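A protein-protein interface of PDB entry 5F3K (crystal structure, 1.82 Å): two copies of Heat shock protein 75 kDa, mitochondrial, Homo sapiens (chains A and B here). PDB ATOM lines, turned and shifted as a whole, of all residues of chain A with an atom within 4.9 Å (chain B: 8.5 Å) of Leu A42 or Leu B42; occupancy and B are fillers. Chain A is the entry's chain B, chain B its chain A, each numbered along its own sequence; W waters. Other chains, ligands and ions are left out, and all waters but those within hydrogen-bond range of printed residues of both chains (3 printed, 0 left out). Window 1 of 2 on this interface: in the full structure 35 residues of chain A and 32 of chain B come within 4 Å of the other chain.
The side-chain hydroxyl (OG1) of Thr B38 lies within hydrogen-bond range of the backbone carbonyl oxygen (O) of Gln B35, at 3.0 Å. OG1 of Thr B38 lies within hydrogen-bond range of O of Phe B34, at 3.2 Å.
Printed residues of chain B within 4 Å of Gln A35: Leu B42 and Ala B46. Lys B40 touches none of the printed residues of chain A. Of the printed residues of chain A, Leu B41 touches Leu A42 (3.996 Å). Leu B42 touches just these residues of chain A: Gln A35 (3.6 Å), Thr A38 (3.8 Å), Lys A39 (3.8 Å) and Leu A42 (3.6 Å). Leu B49 touches none of the printed residues of chain A. Of the printed residues of chain A, Leu B128 touches Leu A41 (3.8 Å) and Leu A131 (3.9 Å). The nearest printed residue of chain A that does not touch Leu B42 is Lys A40 (6.5 Å).
Gln A35 touches Ala B46. Val B45 touches Thr A38 (CG1 to CG2, 3.6 Å). Thr A38 touches Ala B46. CD2 of Leu A41 touches CB of Phe B127, at 3.9 Å. Leu B128 touches Leu A41. Leu A42 touches Leu B42 (CD1 to N, 3.6 Å). Ser B124 touches Ile A44. Ala A46 touches Gln B35 (CB to CD, 3.8 Å). CB of Ala A46 touches OG1 of Thr B38, 3.4 Å away. Leu B131 touches Leu A131.
Gln A35 touches Leu B42, but with the chains exchanged Leu A42 does not touch Gln B35 (5.2 Å). Thr A38 touches Val B45, but with the chains exchanged Val A45 does not touch Thr B38 (4.3 Å). Lys A39 touches Leu B42, but with the chains exchanged Leu A42 does not touch Lys B39 (4.7 Å). Leu A41 touches Leu B131, but with the chains exchanged Leu A131 does not touch Leu B41 (4.05 Å). Of the 22 pairs that touch across the chains among the printed residues, 8 have their exchanged pair printed and touching as well.
OG of Ser B124 lies within hydrogen-bond range of NZ of Lys A40. O of Leu A42 sits at hydrogen-bond distance from OG1 of Thr B38 (3.3 Å). The side-chain amide nitrogen of Gln B35 sits at hydrogen-bond distance from the side-chain carboxylate of Asp A43.
Hydrophobic or aromatic side chains of chain B within 4 Å of the printed part of chain A: Phe B34, Leu B42, Val B45, Ala B46, Phe B127, Leu B128 and Leu B131. Printed residues of chain A that touch a printed residue of chain B: Gln A35, Thr A38, Lys A39, Lys A40, Leu A41, Leu A42, Asp A43, Ile A44, Ala A46 and Leu A131. Hydrophobic or aromatic side chains of chain A within 4 Å of the printed part of chain B: Leu A41, Leu A42, Ile A44, Ala A46 and Leu A131. Among the printed residues, no Asp or Glu carboxylate lies within 4 Å of a Lys or Arg side-chain nitrogen of the other chain.
Water W2 lies within hydrogen-bond range of the side-chain hydroxyl of Thr B38 (2.7 Å), the side-chain amide oxygen of Gln B35 (2.8 Å), the backbone carbonyl oxygen of Leu A42 (3.4 Å) and the backbone NH of Asp A43 (3.4 Å). Water W1 lies within hydrogen-bond range of the side-chain amide oxygen of Gln B35 (2.8 Å) and the side-chain carboxylate of Asp A43 (3.1 Å). Water W3 lies within hydrogen-bond range of N of Ser B124 and NZ of Lys A40.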
ATOM      1  N   GLN A  35      37.365 -11.727  12.560  1.00  0.00           N
ATOM      2  CA  GLN A  35      36.900 -13.111  12.489  1.00  0.00           C
ATOM      3  C   GLN A  35      35.775 -13.315  13.488  1.00  0.00           C
ATOM      4  O   GLN A  35      34.748 -13.902  13.170  1.00  0.00           O
ATOM      5  CB  GLN A  35      38.036 -14.098  12.775  1.00  0.00           C
ATOM      6  CG  GLN A  35      39.026 -14.265  11.644  1.00  0.00           C
ATOM      7  CD  GLN A  35      38.426 -14.950  10.425  1.00  0.00           C
ATOM      8  OE1 GLN A  35      38.617 -14.479   9.309  1.00  0.00           O
ATOM      9  NE2 GLN A  35      37.927 -16.171  10.612  1.00  0.00           N
ATOM     10  N   THR A  38      32.520 -11.355  12.758  1.00  0.00           N
ATOM     11  CA  THR A  38      31.825 -11.949  11.610  1.00  0.00           C
ATOM     12  C   THR A  38      31.104 -13.229  12.040  1.00  0.00           C
ATOM     13  O   THR A  38      29.932 -13.453  11.708  1.00  0.00           O
ATOM     14  CB  THR A  38      32.807 -12.225  10.452  1.00  0.00           C
ATOM     15  OG1 THR A  38      33.360 -10.967  10.012  1.00  0.00           O
ATOM     16  CG2 THR A  38      32.063 -12.893   9.269  1.00  0.00           C
ATOM     17  N   LYS A  39      31.789 -14.028  12.845  1.00  0.00           N
ATOM     18  CA  LYS A  39      31.229 -15.278  13.346  1.00  0.00           C
ATOM     19  C   LYS A  39      29.988 -15.007  14.217  1.00  0.00           C
ATOM     20  O   LYS A  39      28.941 -15.633  14.041  1.00  0.00           O
ATOM     21  CB  LYS A  39      32.301 -16.005  14.156  1.00  0.00           C
ATOM     22  CG  LYS A  39      31.937 -17.375  14.667  1.00  0.00           C
ATOM     23  CD  LYS A  39      33.187 -18.044  15.289  1.00  0.00           C
ATOM     24  CE  LYS A  39      34.361 -18.085  14.307  1.00  0.00           C
ATOM     25  NZ  LYS A  39      35.620 -18.684  14.908  1.00  0.00           N
ATOM     26  N   LYS A  40      30.062 -13.968  15.044  1.00  0.00           N
ATOM     27  CA  LYS A  40      28.944 -13.590  15.895  1.00  0.00           C
ATOM     28  C   LYS A  40      27.743 -13.151  15.066  1.00  0.00           C
ATOM     29  O   LYS A  40      26.602 -13.534  15.353  1.00  0.00           O
ATOM     30  CB  LYS A  40      29.373 -12.465  16.846  1.00  0.00           C
ATOM     31  CG  LYS A  40      28.251 -11.898  17.704  1.00  0.00           C
ATOM     32  CD  LYS A  40      28.830 -10.871  18.687  1.00  0.00           C
ATOM     33  CE  LYS A  40      27.782 -10.400  19.699  1.00  0.00           C
ATOM     34  NZ  LYS A  40      26.774  -9.498  19.081  1.00  0.00           N
ATOM     35  N   LEU A  41      27.995 -12.348  14.037  1.00  0.00           N
ATOM     36  CA  LEU A  41      26.900 -11.879  13.188  1.00  0.00           C
ATOM     37  C   LEU A  41      26.274 -13.047  12.431  1.00  0.00           C
ATOM     38  O   LEU A  41      25.051 -13.112  12.273  1.00  0.00           O
ATOM     39  CB  LEU A  41      27.401 -10.846  12.184  1.00  0.00           C
ATOM     40  CG  LEU A  41      26.358 -10.435  11.136  1.00  0.00           C
ATOM     41  CD1 LEU A  41      25.159  -9.744  11.778  1.00  0.00           C
ATOM     42  CD2 LEU A  41      26.992  -9.534  10.096  1.00  0.00           C
ATOM     43  N   LEU A  42      27.109 -13.951  11.936  1.00  0.00           N
ATOM     44  CA  LEU A  42      26.586 -15.044  11.116  1.00  0.00           C
ATOM     45  C   LEU A  42      25.699 -15.979  11.936  1.00  0.00           C
ATOM     46  O   LEU A  42      24.692 -16.488  11.445  1.00  0.00           O
ATOM     47  CB  LEU A  42      27.716 -15.803  10.412  1.00  0.00           C
ATOM     48  CG  LEU A  42      28.425 -15.066   9.268  1.00  0.00           C
ATOM     49  CD1 LEU A  42      29.720 -15.776   8.858  1.00  0.00           C
ATOM     50  CD2 LEU A  42      27.483 -14.910   8.053  1.00  0.00           C
ATOM     51  N   ASP A  43      26.012 -16.112  13.223  1.00  0.00           N
ATOM     52  CA  ASP A  43      25.160 -16.870  14.140  1.00  0.00           C
ATOM     53  C   ASP A  43      23.817 -16.201  14.397  1.00  0.00           C
ATOM     54  O   ASP A  43      22.771 -16.851  14.344  1.00  0.00           O
ATOM     55  CB  ASP A  43      25.892 -17.119  15.457  1.00  0.00           C
ATOM     56  CG  ASP A  43      24.983 -17.657  16.542  1.00  0.00           C
ATOM     57  OD1 ASP A  43      24.583 -18.834  16.451  1.00  0.00           O
ATOM     58  OD2 ASP A  43      24.626 -16.884  17.464  1.00  0.00           O
ATOM     59  N   ILE A  44      23.833 -14.882  14.555  1.00  0.00           N
ATOM     60  CA  ILE A  44      22.586 -14.119  14.689  1.00  0.00           C
ATOM     61  C   ILE A  44      21.758 -14.247  13.415  1.00  0.00           C
ATOM     62  O   ILE A  44      20.548 -14.464  13.463  1.00  0.00           O
ATOM     63  CB  ILE A  44      22.893 -12.631  14.967  1.00  0.00           C
ATOM     64  CG1 ILE A  44      23.432 -12.468  16.395  1.00  0.00           C
ATOM     65  CG2 ILE A  44      21.681 -11.755  14.695  1.00  0.00           C
ATOM     66  CD1 ILE A  44      24.214 -11.169  16.583  1.00  0.00           C
ATOM     67  N   VAL A  45      22.431 -14.170  12.275  1.00  0.00           N
ATOM     68  CA  VAL A  45      21.746 -14.288  10.981  1.00  0.00           C
ATOM     69  C   VAL A  45      21.161 -15.685  10.730  1.00  0.00           C
ATOM     70  O   VAL A  45      20.031 -15.813  10.217  1.00  0.00           O
ATOM     71  CB  VAL A  45      22.662 -13.861   9.833  1.00  0.00           C
ATOM     72  CG1 VAL A  45      22.046 -14.247   8.486  1.00  0.00           C
ATOM     73  CG2 VAL A  45      22.897 -12.336   9.905  1.00  0.00           C
ATOM     74  N   ALA A  46      21.870 -16.717  11.183  1.00  0.00           N
ATOM     75  CA  ALA A  46      21.377 -18.095  11.024  1.00  0.00           C
ATOM     76  C   ALA A  46      20.068 -18.247  11.794  1.00  0.00           C
ATOM     77  O   ALA A  46      19.108 -18.853  11.309  1.00  0.00           O
ATOM     78  CB  ALA A  46      22.408 -19.095  11.537  1.00  0.00           C
ATOM     79  N   LEU A 131      22.251 -11.903   3.002  1.00  0.00           N
ATOM     80  CA  LEU A 131      23.041 -11.170   3.995  1.00  0.00           C
ATOM     81  C   LEU A 131      23.130  -9.693   3.627  1.00  0.00           C
ATOM     82  O   LEU A 131      22.835  -8.812   4.454  1.00  0.00           O
ATOM     83  CB  LEU A 131      24.447 -11.767   4.096  1.00  0.00           C
ATOM     84  CG  LEU A 131      25.371 -11.214   5.192  1.00  0.00           C
ATOM     85  CD1 LEU A 131      24.706 -11.284   6.564  1.00  0.00           C
ATOM     86  CD2 LEU A 131      26.698 -11.968   5.194  1.00  0.00           C
ATOM     87  N   PHE B  34      20.708 -24.065   8.555  1.00  0.00           N
ATOM     88  CA  PHE B  34      20.890 -22.624   8.501  1.00  0.00           C
ATOM     89  C   PHE B  34      22.206 -22.226   9.177  1.00  0.00           C
ATOM     90  O   PHE B  34      22.932 -21.358   8.690  1.00  0.00           O
ATOM     91  CB  PHE B  34      19.708 -21.879   9.145  1.00  0.00           C
ATOM     92  CG  PHE B  34      18.559 -21.619   8.188  1.00  0.00           C
ATOM     93  CD1 PHE B  34      18.627 -20.579   7.270  1.00  0.00           C
ATOM     94  CD2 PHE B  34      17.478 -22.484   8.131  1.00  0.00           C
ATOM     95  CE1 PHE B  34      17.573 -20.337   6.377  1.00  0.00           C
ATOM     96  CE2 PHE B  34      16.430 -22.250   7.249  1.00  0.00           C
ATOM     97  CZ  PHE B  34      16.476 -21.175   6.375  1.00  0.00           C
ATOM     98  N   GLN B  35      22.504 -22.866  10.302  1.00  0.00           N
ATOM     99  CA  GLN B  35      23.791 -22.660  10.967  1.00  0.00           C
ATOM    100  C   GLN B  35      24.962 -23.002  10.055  1.00  0.00           C
ATOM    101  O   GLN B  35      25.906 -22.213   9.930  1.00  0.00           O
ATOM    102  CB  GLN B  35      23.868 -23.445  12.283  1.00  0.00           C
ATOM    103  CG  GLN B  35      23.116 -22.770  13.447  1.00  0.00           C
ATOM    104  CD  GLN B  35      23.830 -21.546  14.023  1.00  0.00           C
ATOM    105  OE1 GLN B  35      24.975 -21.230  13.661  1.00  0.00           O
ATOM    106  NE2 GLN B  35      23.108 -20.790  14.856  1.00  0.00           N
ATOM    107  N   ALA B  36      24.888 -24.145   9.382  1.00  0.00           N
ATOM    108  CA  ALA B  36      26.012 -24.577   8.549  1.00  0.00           C
ATOM    109  C   ALA B  36      26.201 -23.657   7.338  1.00  0.00           C
ATOM    110  O   ALA B  36      27.320 -23.296   6.995  1.00  0.00           O
ATOM    111  CB  ALA B  36      25.824 -26.034   8.100  1.00  0.00           C
ATOM    112  N   GLU B  37      25.103 -23.286   6.680  1.00  0.00           N
ATOM    113  CA  GLU B  37      25.208 -22.402   5.525  1.00  0.00           C
ATOM    114  C   GLU B  37      25.777 -21.018   5.874  1.00  0.00           C
ATOM    115  O   GLU B  37      26.552 -20.450   5.101  1.00  0.00           O
ATOM    116  CB  GLU B  37      23.859 -22.259   4.822  1.00  0.00           C
ATOM    117  CG  GLU B  37      23.327 -23.562   4.235  1.00  0.00           C
ATOM    118  CD  GLU B  37      24.025 -23.983   2.959  1.00  0.00           C
ATOM    119  OE1 GLU B  37      24.842 -23.198   2.416  1.00  0.00           O
ATOM    120  OE2 GLU B  37      23.712 -25.094   2.468  1.00  0.00           O
ATOM    121  N   THR B  38      25.374 -20.440   7.005  1.00  0.00           N
ATOM    122  CA  THR B  38      25.902 -19.120   7.346  1.00  0.00           C
ATOM    123  C   THR B  38      27.381 -19.198   7.728  1.00  0.00           C
ATOM    124  O   THR B  38      28.175 -18.347   7.343  1.00  0.00           O
ATOM    125  CB  THR B  38      25.142 -18.434   8.517  1.00  0.00           C
ATOM    126  OG1 THR B  38      25.199 -19.261   9.687  1.00  0.00           O
ATOM    127  CG2 THR B  38      23.666 -18.162   8.129  1.00  0.00           C
ATOM    128  N   LYS B  39      27.761 -20.293   8.367  1.00  0.00           N
ATOM    129  CA  LYS B  39      29.177 -20.485   8.712  1.00  0.00           C
ATOM    130  C   LYS B  39      30.083 -20.599   7.494  1.00  0.00           C
ATOM    131  O   LYS B  39      31.266 -20.193   7.535  1.00  0.00           O
ATOM    132  CB  LYS B  39      29.368 -21.700   9.608  1.00  0.00           C
ATOM    133  CG  LYS B  39      28.972 -21.502  11.072  1.00  0.00           C
ATOM    134  CD  LYS B  39      28.959 -22.864  11.763  1.00  0.00           C
ATOM    135  CE  LYS B  39      28.243 -22.833  13.114  1.00  0.00           C
ATOM    136  NZ  LYS B  39      28.346 -24.174  13.792  1.00  0.00           N
ATOM    137  N   LYS B  40      29.535 -21.111   6.399  1.00  0.00           N
ATOM    138  CA  LYS B  40      30.300 -21.188   5.163  1.00  0.00           C
ATOM    139  C   LYS B  40      30.783 -19.816   4.693  1.00  0.00           C
ATOM    140  O   LYS B  40      31.729 -19.729   3.911  1.00  0.00           O
ATOM    141  CB  LYS B  40      29.499 -21.886   4.058  1.00  0.00           C
ATOM    142  CG  LYS B  40      29.397 -23.403   4.244  1.00  0.00           C
ATOM    143  CD  LYS B  40      28.634 -24.060   3.098  1.00  0.00           C
ATOM    144  CE  LYS B  40      29.408 -23.984   1.798  1.00  0.00           C
ATOM    145  NZ  LYS B  40      28.722 -24.746   0.697  1.00  0.00           N
ATOM    146  N   LEU B  41      30.103 -18.756   5.128  1.00  0.00           N
ATOM    147  CA  LEU B  41      30.446 -17.396   4.692  1.00  0.00           C
ATOM    148  C   LEU B  41      31.602 -16.772   5.476  1.00  0.00           C
ATOM    149  O   LEU B  41      31.996 -15.640   5.198  1.00  0.00           O
ATOM    150  CB  LEU B  41      29.227 -16.477   4.792  1.00  0.00           C
ATOM    151  CG  LEU B  41      28.012 -16.933   3.974  1.00  0.00           C
ATOM    152  CD1 LEU B  41      26.951 -15.827   3.994  1.00  0.00           C
ATOM    153  CD2 LEU B  41      28.442 -17.213   2.553  1.00  0.00           C
ATOM    154  N   LEU B  42      31.966 -17.391   6.592  1.00  0.00           N
ATOM    155  CA  LEU B  42      32.895 -16.751   7.530  1.00  0.00           C
ATOM    156  C   LEU B  42      34.130 -16.190   6.828  1.00  0.00           C
ATOM    157  O   LEU B  42      34.483 -15.024   7.006  1.00  0.00           O
ATOM    158  CB  LEU B  42      33.303 -17.731   8.627  1.00  0.00           C
ATOM    159  CG  LEU B  42      34.428 -17.242   9.553  1.00  0.00           C
ATOM    160  CD1 LEU B  42      33.980 -15.977  10.312  1.00  0.00           C
ATOM    161  CD2 LEU B  42      34.791 -18.367  10.520  1.00  0.00           C
ATOM    162  N   ASP B  43      34.820 -17.032   6.060  1.00  0.00           N
ATOM    163  CA  ASP B  43      36.116 -16.644   5.525  1.00  0.00           C
ATOM    164  C   ASP B  43      35.967 -15.549   4.471  1.00  0.00           C
ATOM    165  O   ASP B  43      36.705 -14.568   4.472  1.00  0.00           O
ATOM    166  CB  ASP B  43      36.835 -17.868   4.937  1.00  0.00           C
ATOM    167  CG  ASP B  43      37.620 -18.641   5.985  1.00  0.00           C
ATOM    168  OD1 ASP B  43      37.784 -18.118   7.112  1.00  0.00           O
ATOM    169  OD2 ASP B  43      38.042 -19.784   5.696  1.00  0.00           O
ATOM    170  N   ILE B  44      34.971 -15.696   3.600  1.00  0.00           N
ATOM    171  CA  ILE B  44      34.693 -14.707   2.569  1.00  0.00           C
ATOM    172  C   ILE B  44      34.383 -13.326   3.160  1.00  0.00           C
ATOM    173  O   ILE B  44      34.902 -12.286   2.724  1.00  0.00           O
ATOM    174  CB  ILE B  44      33.488 -15.175   1.721  1.00  0.00           C
ATOM    175  CG1 ILE B  44      33.666 -16.657   1.321  1.00  0.00           C
ATOM    176  CG2 ILE B  44      33.313 -14.272   0.529  1.00  0.00           C
ATOM    177  CD1 ILE B  44      33.499 -17.693   2.497  1.00  0.00           C
ATOM    178  N   VAL B  45      33.475 -13.310   4.117  1.00  0.00           N
ATOM    179  CA  VAL B  45      33.044 -12.061   4.714  1.00  0.00           C
ATOM    180  C   VAL B  45      34.149 -11.435   5.556  1.00  0.00           C
ATOM    181  O   VAL B  45      34.395 -10.222   5.479  1.00  0.00           O
ATOM    182  CB  VAL B  45      31.774 -12.269   5.559  1.00  0.00           C
ATOM    183  CG1 VAL B  45      31.433 -10.980   6.340  1.00  0.00           C
ATOM    184  CG2 VAL B  45      30.609 -12.676   4.643  1.00  0.00           C
ATOM    185  N   ALA B  46      34.791 -12.239   6.395  1.00  0.00           N
ATOM    186  CA  ALA B  46      35.765 -11.672   7.331  1.00  0.00           C
ATOM    187  C   ALA B  46      37.009 -11.169   6.606  1.00  0.00           C
ATOM    188  O   ALA B  46      37.532 -10.100   6.928  1.00  0.00           O
ATOM    189  CB  ALA B  46      36.132 -12.671   8.406  1.00  0.00           C
ATOM    190  N   ARG B  47      37.439 -11.893   5.575  1.00  0.00           N
ATOM    191  CA  ARG B  47      38.610 -11.459   4.807  1.00  0.00           C
ATOM    192  C   ARG B  47      38.285 -10.169   4.077  1.00  0.00           C
ATOM    193  O   ARG B  47      39.128  -9.279   3.969  1.00  0.00           O
ATOM    194  CB  ARG B  47      39.030 -12.519   3.790  1.00  0.00           C
ATOM    195  CG  ARG B  47      39.924 -13.604   4.335  1.00  0.00           C
ATOM    196  CD  ARG B  47      40.219 -14.632   3.228  1.00  0.00           C
ATOM    197  NE  ARG B  47      40.923 -15.813   3.716  1.00  0.00           N
ATOM    198  CZ  ARG B  47      40.537 -17.064   3.478  1.00  0.00           C
ATOM    199  NH1 ARG B  47      39.318 -17.309   3.009  1.00  0.00           N
ATOM    200  NH2 ARG B  47      41.325 -18.075   3.825  1.00  0.00           N
ATOM    201  N   SER B  48      37.085 -10.099   3.511  1.00  0.00           N
ATOM    202  CA  SER B  48      36.679  -8.922   2.757  1.00  0.00           C
ATOM    203  C   SER B  48      36.692  -7.680   3.650  1.00  0.00           C
ATOM    204  O   SER B  48      37.339  -6.663   3.340  1.00  0.00           O
ATOM    205  CB  SER B  48      35.280  -9.134   2.177  1.00  0.00           C
ATOM    206  OG  SER B  48      34.816  -7.962   1.538  1.00  0.00           O
ATOM    207  N   LEU B  49      36.038  -7.792   4.798  1.00  0.00           N
ATOM    208  CA  LEU B  49      35.955  -6.657   5.724  1.00  0.00           C
ATOM    209  C   LEU B  49      37.321  -6.281   6.305  1.00  0.00           C
ATOM    210  O   LEU B  49      37.649  -5.099   6.427  1.00  0.00           O
ATOM    211  CB  LEU B  49      34.947  -6.933   6.840  1.00  0.00           C
ATOM    212  CG  LEU B  49      33.466  -7.010   6.417  1.00  0.00           C
ATOM    213  CD1 LEU B  49      32.562  -7.379   7.584  1.00  0.00           C
ATOM    214  CD2 LEU B  49      32.989  -5.719   5.765  1.00  0.00           C
ATOM    215  N   SER B 124      27.479  -6.069  16.058  1.00  0.00           N
ATOM    216  CA  SER B 124      26.822  -6.908  15.046  1.00  0.00           C
ATOM    217  C   SER B 124      25.947  -6.060  14.125  1.00  0.00           C
ATOM    218  O   SER B 124      25.944  -6.255  12.906  1.00  0.00           O
ATOM    219  CB  SER B 124      26.002  -8.016  15.709  1.00  0.00           C
ATOM    220  OG  SER B 124      26.836  -8.885  16.464  1.00  0.00           O
ATOM    221  N   PHE B 127      28.421  -4.422  11.720  1.00  0.00           N
ATOM    222  CA  PHE B 127      28.851  -5.384  10.700  1.00  0.00           C
ATOM    223  C   PHE B 127      27.755  -5.639   9.664  1.00  0.00           C
ATOM    224  O   PHE B 127      28.026  -5.631   8.462  1.00  0.00           O
ATOM    225  CB  PHE B 127      29.312  -6.694  11.323  1.00  0.00           C
ATOM    226  CG  PHE B 127      30.771  -6.704  11.680  1.00  0.00           C
ATOM    227  CD1 PHE B 127      31.656  -7.528  11.012  1.00  0.00           C
ATOM    228  CD2 PHE B 127      31.272  -5.811  12.618  1.00  0.00           C
ATOM    229  CE1 PHE B 127      33.027  -7.436  11.231  1.00  0.00           C
ATOM    230  CE2 PHE B 127      32.640  -5.765  12.900  1.00  0.00           C
ATOM    231  CZ  PHE B 127      33.520  -6.565  12.183  1.00  0.00           C
ATOM    232  N   LEU B 128      26.512  -5.770  10.117  1.00  0.00           N
ATOM    233  CA  LEU B 128      25.413  -6.017   9.167  1.00  0.00           C
ATOM    234  C   LEU B 128      25.233  -4.801   8.266  1.00  0.00           C
ATOM    235  O   LEU B 128      25.063  -4.921   7.049  1.00  0.00           O
ATOM    236  CB  LEU B 128      24.113  -6.332   9.902  1.00  0.00           C
ATOM    237  CG  LEU B 128      22.924  -6.754   9.030  1.00  0.00           C
ATOM    238  CD1 LEU B 128      23.268  -8.030   8.274  1.00  0.00           C
ATOM    239  CD2 LEU B 128      21.684  -6.953   9.861  1.00  0.00           C
ATOM    240  N   LEU B 131      27.705  -4.554   5.548  1.00  0.00           N
ATOM    241  CA  LEU B 131      27.521  -5.580   4.520  1.00  0.00           C
ATOM    242  C   LEU B 131      26.369  -5.213   3.591  1.00  0.00           C
ATOM    243  O   LEU B 131      26.285  -5.696   2.454  1.00  0.00           O
ATOM    244  CB  LEU B 131      27.278  -6.931   5.181  1.00  0.00           C
ATOM    245  CG  LEU B 131      28.542  -7.485   5.848  1.00  0.00           C
ATOM    246  CD1 LEU B 131      28.234  -8.667   6.741  1.00  0.00           C
ATOM    247  CD2 LEU B 131      29.587  -7.858   4.802  1.00  0.00           C
HETATM  248  O   HOH W   1      26.660 -21.062  15.849  1.00  0.00           O
HETATM  249  O   HOH W   2      26.365 -19.359  12.149  1.00  0.00           O
HETATM  250  O   HOH W   3      26.595  -6.358  18.947  1.00  0.00           O
